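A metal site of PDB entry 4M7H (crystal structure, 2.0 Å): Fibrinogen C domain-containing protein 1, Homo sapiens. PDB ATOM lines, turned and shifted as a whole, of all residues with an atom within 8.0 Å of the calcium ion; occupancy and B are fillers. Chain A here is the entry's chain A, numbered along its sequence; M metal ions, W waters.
OD1 of Asn 164 sits at hydrogen-bond distance from OG of Ser 162 (2.8 Å).
The side-chain carboxylate (OD1) of Asp 160 lies within hydrogen-bond range of the backbone NH (N) of Cys 166.
SG of Cys 179 forms a disulfide with SG of Cys 166, 2.0 Å away.
OG of Ser 162 lies close to OD1 of Asn 178 (3.4 Å).
The backbone NH of Asp 160 is in hydrogen-bond range of the side-chain hydroxyl of Thr 153.
The nearest printed residue that does not touch the calcium ion is Asn 165 (4.2 Å).
The calcium ion is bound by the side-chain carboxylate (OD2) of Asp 158, the side-chain carboxylate (OD2) of Asp 160, the backbone carbonyl oxygen (O) of Asn 164, water W1, the side-chain carboxylate (OD1) of Asp 158, water W2 and the backbone carbonyl oxygen (O) of Ser 162.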
ATOM      1  N   THR A 153      31.571  13.286 -17.868  1.00  0.00           N
ATOM      2  CA  THR A 153      31.226  13.533 -16.470  1.00  0.00           C
ATOM      3  C   THR A 153      30.085  12.642 -15.988  1.00  0.00           C
ATOM      4  O   THR A 153      29.087  12.460 -16.674  1.00  0.00           O
ATOM      5  CB  THR A 153      30.834  15.017 -16.259  1.00  0.00           C
ATOM      6  OG1 THR A 153      32.001  15.832 -16.292  1.00  0.00           O
ATOM      7  CG2 THR A 153      30.117  15.202 -14.931  1.00  0.00           C
ATOM      8  N   ARG A 157      31.958  11.966 -10.578  1.00  0.00           N
ATOM      9  CA  ARG A 157      33.224  12.456 -11.117  1.00  0.00           C
ATOM     10  C   ARG A 157      32.967  13.654 -12.018  1.00  0.00           C
ATOM     11  O   ARG A 157      32.691  13.507 -13.212  1.00  0.00           O
ATOM     12  CB  ARG A 157      33.945  11.351 -11.887  1.00  0.00           C
ATOM     13  CG  ARG A 157      35.412  11.654 -12.206  1.00  0.00           C
ATOM     14  CD  ARG A 157      36.090  10.419 -12.795  1.00  0.00           C
ATOM     15  NE  ARG A 157      37.544  10.549 -12.882  1.00  0.00           N
ATOM     16  CZ  ARG A 157      38.192  11.321 -13.750  1.00  0.00           C
ATOM     17  NH1 ARG A 157      37.528  12.045 -14.639  1.00  0.00           N
ATOM     18  NH2 ARG A 157      39.521  11.358 -13.740  1.00  0.00           N
ATOM     19  N   ASP A 158      33.083  14.844 -11.426  1.00  0.00           N
ATOM     20  CA  ASP A 158      32.851  16.101 -12.120  1.00  0.00           C
ATOM     21  C   ASP A 158      34.056  16.603 -12.909  1.00  0.00           C
ATOM     22  O   ASP A 158      35.128  16.811 -12.349  1.00  0.00           O
ATOM     23  CB  ASP A 158      32.435  17.162 -11.105  1.00  0.00           C
ATOM     24  CG  ASP A 158      31.837  18.398 -11.760  1.00  0.00           C
ATOM     25  OD1 ASP A 158      32.264  18.757 -12.883  1.00  0.00           O
ATOM     26  OD2 ASP A 158      30.951  19.017 -11.139  1.00  0.00           O
ATOM     27  N   SER A 159      33.858  16.814 -14.204  1.00  0.00           N
ATOM     28  CA  SER A 159      34.907  17.322 -15.087  1.00  0.00           C
ATOM     29  C   SER A 159      34.301  18.271 -16.115  1.00  0.00           C
ATOM     30  O   SER A 159      34.879  18.469 -17.190  1.00  0.00           O
ATOM     31  CB  SER A 159      35.617  16.167 -15.804  1.00  0.00           C
ATOM     32  OG  SER A 159      36.315  15.334 -14.891  1.00  0.00           O
ATOM     33  N   ASP A 160      33.148  18.848 -15.791  1.00  0.00           N
ATOM     34  CA  ASP A 160      32.470  19.751 -16.707  1.00  0.00           C
ATOM     35  C   ASP A 160      32.824  21.215 -16.473  1.00  0.00           C
ATOM     36  O   ASP A 160      33.652  21.529 -15.612  1.00  0.00           O
ATOM     37  CB  ASP A 160      30.945  19.558 -16.602  1.00  0.00           C
ATOM     38  CG  ASP A 160      30.412  19.883 -15.214  1.00  0.00           C
ATOM     39  OD1 ASP A 160      29.568  19.114 -14.711  1.00  0.00           O
ATOM     40  OD2 ASP A 160      30.821  20.909 -14.634  1.00  0.00           O
ATOM     41  N   HIS A 161      32.210  22.110 -17.242  1.00  0.00           N
ATOM     42  CA  HIS A 161      32.467  23.531 -17.108  1.00  0.00           C
ATOM     43  C   HIS A 161      31.378  24.240 -16.313  1.00  0.00           C
ATOM     44  O   HIS A 161      31.136  25.438 -16.497  1.00  0.00           O
ATOM     45  CB  HIS A 161      32.602  24.190 -18.482  1.00  0.00           C
ATOM     46  CG  HIS A 161      33.928  23.960 -19.137  1.00  0.00           C
ATOM     47  ND1 HIS A 161      34.336  24.654 -20.255  1.00  0.00           N
ATOM     48  CD2 HIS A 161      34.942  23.108 -18.825  1.00  0.00           C
ATOM     49  CE1 HIS A 161      35.542  24.236 -20.612  1.00  0.00           C
ATOM     50  NE2 HIS A 161      35.932  23.305 -19.756  1.00  0.00           N
ATOM     51  N   SER A 162      30.717  23.492 -15.438  1.00  0.00           N
ATOM     52  CA  SER A 162      29.644  24.038 -14.612  1.00  0.00           C
ATOM     53  C   SER A 162      30.089  24.179 -13.163  1.00  0.00           C
ATOM     54  O   SER A 162      30.998  23.488 -12.704  1.00  0.00           O
ATOM     55  CB  SER A 162      28.413  23.140 -14.685  1.00  0.00           C
ATOM     56  OG  SER A 162      27.396  23.596 -13.803  1.00  0.00           O
ATOM     57  N   GLU A 163      29.437  25.097 -12.448  1.00  0.00           N
ATOM     58  CA  GLU A 163      29.734  25.351 -11.047  1.00  0.00           C
ATOM     59  C   GLU A 163      29.344  24.122 -10.230  1.00  0.00           C
ATOM     60  O   GLU A 163      29.906  23.850  -9.174  1.00  0.00           O
ATOM     61  CB  GLU A 163      28.963  26.580 -10.561  1.00  0.00           C
ATOM     62  CG  GLU A 163      29.089  27.803 -11.464  1.00  0.00           C
ATOM     63  CD  GLU A 163      28.472  27.593 -12.841  1.00  0.00           C
ATOM     64  OE1 GLU A 163      27.266  27.270 -12.926  1.00  0.00           O
ATOM     65  OE2 GLU A 163      29.195  27.748 -13.854  1.00  0.00           O
ATOM     66  N   ASN A 164      28.354  23.392 -10.738  1.00  0.00           N
ATOM     67  CA  ASN A 164      27.872  22.182 -10.069  1.00  0.00           C
ATOM     68  C   ASN A 164      28.158  20.969 -10.953  1.00  0.00           C
ATOM     69  O   ASN A 164      28.890  21.059 -11.934  1.00  0.00           O
ATOM     70  CB  ASN A 164      26.380  22.294  -9.795  1.00  0.00           C
ATOM     71  CG  ASN A 164      25.587  22.739 -11.006  1.00  0.00           C
ATOM     72  OD1 ASN A 164      25.795  23.833 -11.533  1.00  0.00           O
ATOM     73  ND2 ASN A 164      24.682  21.888 -11.469  1.00  0.00           N
ATOM     74  N   ASN A 165      27.576  19.829 -10.593  1.00  0.00           N
ATOM     75  CA  ASN A 165      27.780  18.607 -11.361  1.00  0.00           C
ATOM     76  C   ASN A 165      26.611  18.413 -12.329  1.00  0.00           C
ATOM     77  O   ASN A 165      25.513  18.048 -11.933  1.00  0.00           O
ATOM     78  CB  ASN A 165      27.872  17.398 -10.424  1.00  0.00           C
ATOM     79  CG  ASN A 165      28.217  16.120 -11.148  1.00  0.00           C
ATOM     80  OD1 ASN A 165      27.566  15.740 -12.120  1.00  0.00           O
ATOM     81  ND2 ASN A 165      29.259  15.434 -10.686  1.00  0.00           N
ATOM     82  N   CYS A 166      26.871  18.675 -13.604  1.00  0.00           N
ATOM     83  CA  CYS A 166      25.844  18.540 -14.637  1.00  0.00           C
ATOM     84  C   CYS A 166      25.213  17.147 -14.644  1.00  0.00           C
ATOM     85  O   CYS A 166      23.998  17.019 -14.817  1.00  0.00           O
ATOM     86  CB  CYS A 166      26.428  18.824 -16.019  1.00  0.00           C
ATOM     87  SG  CYS A 166      26.934  20.535 -16.395  1.00  0.00           S
ATOM     88  N   ALA A 167      26.035  16.118 -14.490  1.00  0.00           N
ATOM     89  CA  ALA A 167      25.554  14.739 -14.494  1.00  0.00           C
ATOM     90  C   ALA A 167      24.494  14.488 -13.423  1.00  0.00           C
ATOM     91  O   ALA A 167      23.506  13.791 -13.662  1.00  0.00           O
ATOM     92  CB  ALA A 167      26.719  13.766 -14.322  1.00  0.00           C
ATOM     93  N   TYR A 176      29.463  16.677 -20.726  1.00  0.00           N
ATOM     94  CA  TYR A 176      28.862  17.938 -20.329  1.00  0.00           C
ATOM     95  C   TYR A 176      29.765  19.148 -20.411  1.00  0.00           C
ATOM     96  O   TYR A 176      30.966  19.078 -20.131  1.00  0.00           O
ATOM     97  CB  TYR A 176      28.338  17.813 -18.898  1.00  0.00           C
ATOM     98  CG  TYR A 176      27.195  16.832 -18.738  1.00  0.00           C
ATOM     99  CD1 TYR A 176      25.963  17.059 -19.346  1.00  0.00           C
ATOM    100  CD2 TYR A 176      27.340  15.709 -17.937  1.00  0.00           C
ATOM    101  CE1 TYR A 176      24.898  16.186 -19.156  1.00  0.00           C
ATOM    102  CE2 TYR A 176      26.275  14.831 -17.733  1.00  0.00           C
ATOM    103  CZ  TYR A 176      25.057  15.076 -18.344  1.00  0.00           C
ATOM    104  OH  TYR A 176      23.997  14.231 -18.131  1.00  0.00           O
ATOM    105  N   ARG A 177      29.165  20.274 -20.780  1.00  0.00           N
ATOM    106  CA  ARG A 177      29.857  21.540 -20.869  1.00  0.00           C
ATOM    107  C   ARG A 177      29.245  22.383 -19.757  1.00  0.00           C
ATOM    108  O   ARG A 177      29.717  22.379 -18.621  1.00  0.00           O
ATOM    109  CB  ARG A 177      29.630  22.195 -22.223  1.00  0.00           C
ATOM    110  CG  ARG A 177      30.494  23.411 -22.477  1.00  0.00           C
ATOM    111  CD  ARG A 177      30.260  23.996 -23.858  1.00  0.00           C
ATOM    112  NE  ARG A 177      31.192  25.069 -24.154  1.00  0.00           N
ATOM    113  CZ  ARG A 177      32.510  24.904 -24.263  1.00  0.00           C
ATOM    114  NH1 ARG A 177      33.050  23.701 -24.103  1.00  0.00           N
ATOM    115  NH2 ARG A 177      33.298  25.944 -24.517  1.00  0.00           N
ATOM    116  N   ASN A 178      28.165  23.083 -20.078  1.00  0.00           N
ATOM    117  CA  ASN A 178      27.478  23.909 -19.082  1.00  0.00           C
ATOM    118  C   ASN A 178      26.067  24.268 -19.552  1.00  0.00           C
ATOM    119  O   ASN A 178      25.773  25.443 -19.797  1.00  0.00           O
ATOM    120  CB  ASN A 178      28.294  25.184 -18.811  1.00  0.00           C
ATOM    121  CG  ASN A 178      27.721  26.013 -17.670  1.00  0.00           C
ATOM    122  OD1 ASN A 178      27.459  25.497 -16.588  1.00  0.00           O
ATOM    123  ND2 ASN A 178      27.527  27.301 -17.914  1.00  0.00           N
ATOM    124  N   CYS A 179      25.199  23.268 -19.678  1.00  0.00           N
ATOM    125  CA  CYS A 179      25.548  21.880 -19.412  1.00  0.00           C
ATOM    126  C   CYS A 179      25.476  20.970 -20.637  1.00  0.00           C
ATOM    127  O   CYS A 179      26.357  20.146 -20.852  1.00  0.00           O
ATOM    128  CB  CYS A 179      24.664  21.293 -18.311  1.00  0.00           C
ATOM    129  SG  CYS A 179      25.185  21.563 -16.580  1.00  0.00           S
HETATM  130 CA    CA M   1      31.274  20.945 -12.321  1.00  0.00          CA
HETATM  131  O   HOH W   1      33.566  21.521 -12.961  1.00  0.00           O
HETATM  132  O   HOH W   2      32.184  21.691 -10.133  1.00  0.00           O
